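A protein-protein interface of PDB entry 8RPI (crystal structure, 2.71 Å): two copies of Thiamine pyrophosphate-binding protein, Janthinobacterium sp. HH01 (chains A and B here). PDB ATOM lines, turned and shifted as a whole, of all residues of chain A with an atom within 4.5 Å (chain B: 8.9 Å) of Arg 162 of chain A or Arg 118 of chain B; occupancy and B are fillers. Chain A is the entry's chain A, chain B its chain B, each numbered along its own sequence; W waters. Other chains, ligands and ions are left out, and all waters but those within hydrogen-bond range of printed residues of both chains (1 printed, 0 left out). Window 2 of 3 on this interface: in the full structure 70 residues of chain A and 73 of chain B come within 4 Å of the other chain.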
ATOM      1  N   TRP A  93      10.914 -14.009  21.924  1.00  0.00           N
ATOM      2  CA  TRP A  93      10.779 -14.266  20.497  1.00  0.00           C
ATOM      3  C   TRP A  93       9.337 -14.090  20.053  1.00  0.00           C
ATOM      4  O   TRP A  93       9.068 -13.449  19.029  1.00  0.00           O
ATOM      5  CB  TRP A  93      11.293 -15.677  20.212  1.00  0.00           C
ATOM      6  CG  TRP A  93      10.985 -16.276  18.876  1.00  0.00           C
ATOM      7  CD1 TRP A  93      10.053 -17.234  18.607  1.00  0.00           C
ATOM      8  CD2 TRP A  93      11.647 -16.004  17.640  1.00  0.00           C
ATOM      9  NE1 TRP A  93      10.084 -17.565  17.277  1.00  0.00           N
ATOM     10  CE2 TRP A  93      11.056 -16.822  16.660  1.00  0.00           C
ATOM     11  CE3 TRP A  93      12.678 -15.141  17.265  1.00  0.00           C
ATOM     12  CZ2 TRP A  93      11.460 -16.801  15.330  1.00  0.00           C
ATOM     13  CZ3 TRP A  93      13.076 -15.119  15.943  1.00  0.00           C
ATOM     14  CH2 TRP A  93      12.468 -15.942  14.991  1.00  0.00           C
ATOM     15  N   ALA A  94       8.394 -14.611  20.836  1.00  0.00           N
ATOM     16  CA  ALA A  94       6.990 -14.546  20.458  1.00  0.00           C
ATOM     17  C   ALA A  94       6.431 -13.132  20.563  1.00  0.00           C
ATOM     18  O   ALA A  94       5.524 -12.772  19.803  1.00  0.00           O
ATOM     19  CB  ALA A  94       6.177 -15.496  21.336  1.00  0.00           C
ATOM     20  N   SER A  96       8.264 -10.258  20.265  1.00  0.00           N
ATOM     21  CA  SER A  96       9.039  -9.295  19.484  1.00  0.00           C
ATOM     22  C   SER A  96       9.771  -8.304  20.385  1.00  0.00           C
ATOM     23  O   SER A  96       9.828  -7.109  20.098  1.00  0.00           O
ATOM     24  CB  SER A  96       8.143  -8.550  18.493  1.00  0.00           C
ATOM     25  OG  SER A  96       7.311  -9.444  17.780  1.00  0.00           O
ATOM     26  N   LYS A 136      16.541 -14.560  16.796  1.00  0.00           N
ATOM     27  CA  LYS A 136      16.861 -13.894  15.543  1.00  0.00           C
ATOM     28  C   LYS A 136      18.274 -14.180  15.056  1.00  0.00           C
ATOM     29  O   LYS A 136      18.534 -14.073  13.852  1.00  0.00           O
ATOM     30  CB  LYS A 136      16.677 -12.385  15.694  1.00  0.00           C
ATOM     31  CG  LYS A 136      15.237 -11.966  15.926  1.00  0.00           C
ATOM     32  CD  LYS A 136      15.067 -10.454  15.875  1.00  0.00           C
ATOM     33  CE  LYS A 136      15.459  -9.884  14.519  1.00  0.00           C
ATOM     34  NZ  LYS A 136      15.276  -8.415  14.446  1.00  0.00           N
ATOM     35  N   GLU A 160      16.886  -4.599  15.299  1.00  0.00           N
ATOM     36  CA  GLU A 160      16.546  -4.368  13.904  1.00  0.00           C
ATOM     37  C   GLU A 160      15.172  -4.943  13.572  1.00  0.00           C
ATOM     38  O   GLU A 160      14.723  -5.931  14.162  1.00  0.00           O
ATOM     39  CB  GLU A 160      17.620  -4.989  13.007  1.00  0.00           C
ATOM     40  CG  GLU A 160      17.266  -5.091  11.537  1.00  0.00           C
ATOM     41  CD  GLU A 160      16.454  -6.325  11.205  1.00  0.00           C
ATOM     42  OE1 GLU A 160      16.415  -7.263  12.033  1.00  0.00           O
ATOM     43  OE2 GLU A 160      15.851  -6.350  10.111  1.00  0.00           O
ATOM     44  N   GLY A 161      14.508  -4.308  12.606  1.00  0.00           N
ATOM     45  CA  GLY A 161      13.268  -4.810  12.050  1.00  0.00           C
ATOM     46  C   GLY A 161      12.279  -5.257  13.100  1.00  0.00           C
ATOM     47  O   GLY A 161      11.903  -4.483  13.985  1.00  0.00           O
ATOM     48  N   ARG A 162      11.845  -6.508  13.006  1.00  0.00           N
ATOM     49  CA  ARG A 162      10.989  -7.078  14.033  1.00  0.00           C
ATOM     50  C   ARG A 162      11.881  -7.481  15.199  1.00  0.00           C
ATOM     51  O   ARG A 162      12.664  -8.430  15.072  1.00  0.00           O
ATOM     52  CB  ARG A 162      10.209  -8.278  13.507  1.00  0.00           C
ATOM     53  CG  ARG A 162       9.259  -8.850  14.535  1.00  0.00           C
ATOM     54  CD  ARG A 162       8.497 -10.035  13.995  1.00  0.00           C
ATOM     55  NE  ARG A 162       7.598 -10.587  14.998  1.00  0.00           N
ATOM     56  CZ  ARG A 162       6.770 -11.600  14.785  1.00  0.00           C
ATOM     57  NH1 ARG A 162       6.734 -12.229  13.621  1.00  0.00           N
ATOM     58  NH2 ARG A 162       5.955 -11.987  15.759  1.00  0.00           N
ATOM     59  N   PRO A 163      11.810  -6.795  16.339  1.00  0.00           N
ATOM     60  CA  PRO A 163      12.763  -7.075  17.419  1.00  0.00           C
ATOM     61  C   PRO A 163      12.595  -8.483  17.960  1.00  0.00           C
ATOM     62  O   PRO A 163      11.595  -9.161  17.720  1.00  0.00           O
ATOM     63  CB  PRO A 163      12.428  -6.024  18.483  1.00  0.00           C
ATOM     64  CG  PRO A 163      11.617  -4.986  17.776  1.00  0.00           C
ATOM     65  CD  PRO A 163      10.877  -5.715  16.705  1.00  0.00           C
ATOM     66  N   GLY A 164      13.607  -8.919  18.712  1.00  0.00           N
ATOM     67  CA  GLY A 164      13.624 -10.241  19.291  1.00  0.00           C
ATOM     68  C   GLY A 164      14.972 -10.582  19.897  1.00  0.00           C
ATOM     69  O   GLY A 164      15.950  -9.845  19.745  1.00  0.00           O
ATOM     70  N   ARG A 290      -0.522  -7.882  15.529  1.00  0.00           N
ATOM     71  CA  ARG A 290      -0.313  -9.154  14.852  1.00  0.00           C
ATOM     72  C   ARG A 290      -1.608  -9.811  14.396  1.00  0.00           C
ATOM     73  O   ARG A 290      -1.558 -10.758  13.602  1.00  0.00           O
ATOM     74  CB  ARG A 290       0.444 -10.105  15.784  1.00  0.00           C
ATOM     75  CG  ARG A 290       0.980 -11.363  15.118  1.00  0.00           C
ATOM     76  CD  ARG A 290       2.087 -12.010  15.953  1.00  0.00           C
ATOM     77  NE  ARG A 290       1.683 -12.275  17.330  1.00  0.00           N
ATOM     78  CZ  ARG A 290       1.152 -13.414  17.758  1.00  0.00           C
ATOM     79  NH1 ARG A 290       0.937 -14.430  16.939  1.00  0.00           N
ATOM     80  NH2 ARG A 290       0.830 -13.535  19.043  1.00  0.00           N
ATOM     81  N   ILE A 314       5.860  -4.706  10.190  1.00  0.00           N
ATOM     82  CA  ILE A 314       7.229  -4.699   9.675  1.00  0.00           C
ATOM     83  C   ILE A 314       7.714  -6.076   9.252  1.00  0.00           C
ATOM     84  O   ILE A 314       8.773  -6.184   8.621  1.00  0.00           O
ATOM     85  CB  ILE A 314       8.177  -4.106  10.735  1.00  0.00           C
ATOM     86  CG1 ILE A 314       9.468  -3.625  10.077  1.00  0.00           C
ATOM     87  CG2 ILE A 314       8.470  -5.122  11.839  1.00  0.00           C
ATOM     88  CD1 ILE A 314      10.365  -2.878  11.016  1.00  0.00           C
ATOM     89  N   ASP A 315       6.972  -7.127   9.579  1.00  0.00           N
ATOM     90  CA  ASP A 315       7.323  -8.494   9.223  1.00  0.00           C
ATOM     91  C   ASP A 315       6.476  -8.910   8.024  1.00  0.00           C
ATOM     92  O   ASP A 315       5.244  -8.929   8.108  1.00  0.00           O
ATOM     93  CB  ASP A 315       7.091  -9.418  10.419  1.00  0.00           C
ATOM     94  CG  ASP A 315       7.689 -10.793  10.232  1.00  0.00           C
ATOM     95  OD1 ASP A 315       7.702 -11.298   9.089  1.00  0.00           O
ATOM     96  OD2 ASP A 315       8.142 -11.372  11.243  1.00  0.00           O
ATOM     97  N   GLU A 318       4.075 -11.874   8.654  1.00  0.00           N
ATOM     98  CA  GLU A 318       2.906 -11.521   9.456  1.00  0.00           C
ATOM     99  C   GLU A 318       1.945 -10.624   8.680  1.00  0.00           C
ATOM    100  O   GLU A 318       0.738 -10.631   8.949  1.00  0.00           O
ATOM    101  CB  GLU A 318       3.339 -10.831  10.753  1.00  0.00           C
ATOM    102  CG  GLU A 318       4.228 -11.663  11.675  1.00  0.00           C
ATOM    103  CD  GLU A 318       3.488 -12.777  12.388  1.00  0.00           C
ATOM    104  OE1 GLU A 318       2.246 -12.842  12.277  1.00  0.00           O
ATOM    105  OE2 GLU A 318       4.155 -13.586  13.067  1.00  0.00           O
ATOM    106  N   ASN B 115       6.214 -23.676   8.509  1.00  0.00           N
ATOM    107  CA  ASN B 115       5.368 -22.560   8.899  1.00  0.00           C
ATOM    108  C   ASN B 115       6.203 -21.285   8.943  1.00  0.00           C
ATOM    109  O   ASN B 115       7.164 -21.210   9.726  1.00  0.00           O
ATOM    110  CB  ASN B 115       4.733 -22.821  10.258  1.00  0.00           C
ATOM    111  CG  ASN B 115       3.625 -21.840  10.574  1.00  0.00           C
ATOM    112  OD1 ASN B 115       3.628 -20.709  10.093  1.00  0.00           O
ATOM    113  ND2 ASN B 115       2.667 -22.271  11.382  1.00  0.00           N
ATOM    114  N   PRO B 116       5.880 -20.268   8.137  1.00  0.00           N
ATOM    115  CA  PRO B 116       6.744 -19.079   8.071  1.00  0.00           C
ATOM    116  C   PRO B 116       6.640 -18.162   9.276  1.00  0.00           C
ATOM    117  O   PRO B 116       7.425 -17.206   9.364  1.00  0.00           O
ATOM    118  CB  PRO B 116       6.258 -18.371   6.802  1.00  0.00           C
ATOM    119  CG  PRO B 116       4.820 -18.755   6.692  1.00  0.00           C
ATOM    120  CD  PRO B 116       4.700 -20.144   7.260  1.00  0.00           C
ATOM    121  N   LEU B 117       5.715 -18.411  10.196  1.00  0.00           N
ATOM    122  CA  LEU B 117       5.519 -17.544  11.346  1.00  0.00           C
ATOM    123  C   LEU B 117       6.439 -17.952  12.494  1.00  0.00           C
ATOM    124  O   LEU B 117       6.884 -19.097  12.592  1.00  0.00           O
ATOM    125  CB  LEU B 117       4.057 -17.579  11.799  1.00  0.00           C
ATOM    126  CG  LEU B 117       3.017 -17.169  10.748  1.00  0.00           C
ATOM    127  CD1 LEU B 117       1.615 -17.132  11.351  1.00  0.00           C
ATOM    128  CD2 LEU B 117       3.362 -15.829  10.109  1.00  0.00           C
ATOM    129  N   ARG B 118       6.722 -16.979  13.368  1.00  0.00           N
ATOM    130  CA  ARG B 118       7.620 -17.215  14.494  1.00  0.00           C
ATOM    131  C   ARG B 118       7.087 -18.287  15.429  1.00  0.00           C
ATOM    132  O   ARG B 118       7.870 -18.978  16.094  1.00  0.00           O
ATOM    133  CB  ARG B 118       7.832 -15.923  15.287  1.00  0.00           C
ATOM    134  CG  ARG B 118       8.755 -14.914  14.637  1.00  0.00           C
ATOM    135  CD  ARG B 118       9.288 -13.939  15.665  1.00  0.00           C
ATOM    136  NE  ARG B 118      10.225 -12.996  15.069  1.00  0.00           N
ATOM    137  CZ  ARG B 118      10.754 -11.959  15.702  1.00  0.00           C
ATOM    138  NH1 ARG B 118      10.461 -11.694  16.964  1.00  0.00           N
ATOM    139  NH2 ARG B 118      11.598 -11.167  15.049  1.00  0.00           N
ATOM    140  N   MET B 119       5.767 -18.416  15.517  1.00  0.00           N
ATOM    141  CA  MET B 119       5.138 -19.359  16.426  1.00  0.00           C
ATOM    142  C   MET B 119       4.002 -20.065  15.701  1.00  0.00           C
ATOM    143  O   MET B 119       3.501 -19.592  14.680  1.00  0.00           O
ATOM    144  CB  MET B 119       4.613 -18.662  17.688  1.00  0.00           C
ATOM    145  CG  MET B 119       5.697 -17.981  18.521  1.00  0.00           C
ATOM    146  SD  MET B 119       6.773 -19.131  19.404  1.00  0.00           S
ATOM    147  CE  MET B 119       5.635 -19.767  20.636  1.00  0.00           C
ATOM    148  N   TRP B 120       3.604 -21.205  16.252  1.00  0.00           N
ATOM    149  CA  TRP B 120       2.583 -22.060  15.661  1.00  0.00           C
ATOM    150  C   TRP B 120       1.263 -21.843  16.383  1.00  0.00           C
ATOM    151  O   TRP B 120       1.214 -21.874  17.615  1.00  0.00           O
ATOM    152  CB  TRP B 120       2.989 -23.533  15.753  1.00  0.00           C
ATOM    153  CG  TRP B 120       4.185 -23.899  14.933  1.00  0.00           C
ATOM    154  CD1 TRP B 120       4.834 -23.112  14.030  1.00  0.00           C
ATOM    155  CD2 TRP B 120       4.875 -25.152  14.942  1.00  0.00           C
ATOM    156  NE1 TRP B 120       5.887 -23.797  13.476  1.00  0.00           N
ATOM    157  CE2 TRP B 120       5.932 -25.054  14.020  1.00  0.00           C
ATOM    158  CE3 TRP B 120       4.702 -26.348  15.641  1.00  0.00           C
ATOM    159  CZ2 TRP B 120       6.807 -26.107  13.778  1.00  0.00           C
ATOM    160  CZ3 TRP B 120       5.569 -27.391  15.396  1.00  0.00           C
ATOM    161  CH2 TRP B 120       6.607 -27.265  14.475  1.00  0.00           C
ATOM    162  N   GLY B 121       0.197 -21.641  15.614  1.00  0.00           N
ATOM    163  CA  GLY B 121      -1.106 -21.402  16.199  1.00  0.00           C
ATOM    164  C   GLY B 121      -1.091 -20.278  17.216  1.00  0.00           C
ATOM    165  O   GLY B 121      -0.710 -19.146  16.901  1.00  0.00           O
ATOM    166  N   VAL B 122      -1.493 -20.584  18.444  1.00  0.00           N
ATOM    167  CA  VAL B 122      -1.591 -19.573  19.491  1.00  0.00           C
ATOM    168  C   VAL B 122      -0.277 -19.425  20.243  1.00  0.00           C
ATOM    169  O   VAL B 122       0.234 -18.314  20.403  1.00  0.00           O
ATOM    170  CB  VAL B 122      -2.753 -19.920  20.449  1.00  0.00           C
ATOM    171  CG1 VAL B 122      -2.894 -18.849  21.527  1.00  0.00           C
ATOM    172  CG2 VAL B 122      -4.066 -20.078  19.680  1.00  0.00           C
ATOM    173  N   GLN B 123       0.299 -20.541  20.716  1.00  0.00           N
ATOM    174  CA  GLN B 123       1.505 -20.467  21.533  1.00  0.00           C
ATOM    175  C   GLN B 123       2.413 -21.676  21.333  1.00  0.00           C
ATOM    176  O   GLN B 123       3.077 -22.114  22.280  1.00  0.00           O
ATOM    177  CB  GLN B 123       1.127 -20.337  23.013  1.00  0.00           C
ATOM    178  CG  GLN B 123       0.187 -21.425  23.509  1.00  0.00           C
ATOM    179  CD  GLN B 123      -0.316 -21.156  24.913  1.00  0.00           C
ATOM    180  OE1 GLN B 123      -0.758 -20.049  25.226  1.00  0.00           O
ATOM    181  NE2 GLN B 123      -0.241 -22.165  25.770  1.00  0.00           N
ATOM    182  N   GLY B 124       2.472 -22.215  20.117  1.00  0.00           N
ATOM    183  CA  GLY B 124       3.207 -23.440  19.873  1.00  0.00           C
ATOM    184  C   GLY B 124       4.523 -23.261  19.142  1.00  0.00           C
ATOM    185  O   GLY B 124       4.733 -22.260  18.452  1.00  0.00           O
ATOM    186  N   TYR B 125       5.419 -24.235  19.281  1.00  0.00           N
ATOM    187  CA  TYR B 125       6.692 -24.226  18.574  1.00  0.00           C
ATOM    188  C   TYR B 125       7.051 -25.668  18.244  1.00  0.00           C
ATOM    189  O   TYR B 125       6.366 -26.609  18.658  1.00  0.00           O
ATOM    190  CB  TYR B 125       7.792 -23.554  19.406  1.00  0.00           C
ATOM    191  CG  TYR B 125       8.268 -24.402  20.562  1.00  0.00           C
ATOM    192  CD1 TYR B 125       7.468 -24.603  21.675  1.00  0.00           C
ATOM    193  CD2 TYR B 125       9.515 -25.005  20.537  1.00  0.00           C
ATOM    194  CE1 TYR B 125       7.894 -25.384  22.735  1.00  0.00           C
ATOM    195  CE2 TYR B 125       9.956 -25.783  21.595  1.00  0.00           C
ATOM    196  CZ  TYR B 125       9.137 -25.974  22.691  1.00  0.00           C
ATOM    197  OH  TYR B 125       9.560 -26.749  23.749  1.00  0.00           O
ATOM    198  N   ASP B 126       8.136 -25.836  17.490  1.00  0.00           N
ATOM    199  CA  ASP B 126       8.636 -27.161  17.130  1.00  0.00           C
ATOM    200  C   ASP B 126       9.388 -27.715  18.329  1.00  0.00           C
ATOM    201  O   ASP B 126      10.603 -27.561  18.451  1.00  0.00           O
ATOM    202  CB  ASP B 126       9.532 -27.086  15.902  1.00  0.00           C
ATOM    203  CG  ASP B 126       9.858 -28.451  15.328  1.00  0.00           C
ATOM    204  OD1 ASP B 126       9.742 -29.460  16.058  1.00  0.00           O
ATOM    205  OD2 ASP B 126      10.240 -28.511  14.142  1.00  0.00           O
HETATM  206  O   HOH W   1       1.046 -17.422  17.623  1.00  0.00           O
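The backbone carbonyl oxygen (O) of Arg 162 of chain A sits at hydrogen-bond distance from the guanidinium group (NH2) of Arg 118 of chain B, 2.9 Å away.
NE1 of Trp 93 of chain A lies within hydrogen-bond range of O of Arg 118 of chain B (2.9 Å).
The backbone carbonyl oxygen (O) of Pro 163 of chain A sits at hydrogen-bond distance from the guanidinium group (NH1) of Arg 118 of chain B (2.9 Å).
OG of Ser 96 of chain A is in hydrogen-bond range of NE of Arg 162 of chain A (3.0 Å).
N of Leu 117 of chain B lies within hydrogen-bond range of OD1 of Asn 115 of chain B (3.1 Å).
NH1 of Arg 162 of chain A is in salt-bridge range of OD2 of Asp 315 of chain A, at 2.9 Å.
O of Arg 162 of chain A lies within hydrogen-bond range of NZ of Lys 136 of chain A, 2.7 Å away.
OE2 of Glu 318 of chain A is in salt-bridge range of NH1 of Arg 162 of chain A, at 3.0 Å.
The side-chain amino group of Lys 136 of chain A lies within salt-bridge range of the side-chain carboxylate of Glu 160 of chain A (2.9 Å).
Trp 93 of chain A touches Met 119 of chain B (CD1 to SD, 3.9 Å).
Met 119 of chain B touches Ala 94 of chain A (CG to CB, 3.8 Å).
CA of Ser 96 of chain A touches NH1 of Arg 118 of chain B (3.8 Å).
CD of Lys 136 of chain A touches NH2 of Arg 118 of chain B (3.6 Å).
Leu 117 of chain B touches Glu 318 of chain A (CD2 to OE2, 3.8 Å).
Of the printed residues of chain B, Ala 94 of chain A touches Met 119 (3.8 Å).
Of the printed residues of chain B, Lys 136 of chain A touches Arg 118 (3.6 Å).
Of chain B, only Arg 118 (2.9 Å) comes within 4 Å of Pro 163 of chain A.
Printed residues of chain B within 4 Å of Glu 318 of chain A: Leu 117.
Of the printed residues of chain A, Arg 118 of chain B touches Trp 93 (2.9 Å), Ser 96 (3.8 Å), Lys 136 (3.6 Å), Arg 162 (2.9 Å) and Pro 163 (2.9 Å).
Val 122 of chain B touches none of the printed residues of chain A.
The nearest residue of chain B that does not touch Arg 162 of chain A is Leu 117 of chain B (5.8 Å).
The nearest residue of chain A that does not touch Arg 118 of chain B is Gly 164 of chain A (4.2 Å).
Hydrophobic or aromatic side chains of chain B within 4 Å of the printed part of chain A: Leu 117 and Met 119.
Hydrophobic or aromatic side chains of chain A that line the printed part of chain B: Trp 93 and Ala 94.
Among the printed residues, no Asp or Glu carboxylate lies within 4 Å of a Lys or Arg side-chain nitrogen of the other chain.
No position is printed for both chains.
Of the 8 pairs that touch across the chains among the printed residues, none has its exchanged pair printed and touching as well.
Water W1 lies within hydrogen-bond range of the backbone carbonyl oxygen (O) of Gly 121 of chain B, the backbone carbonyl oxygen (O) of Val 122 of chain B and the guanidinium group (NH1) of Arg 290 of chain A.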
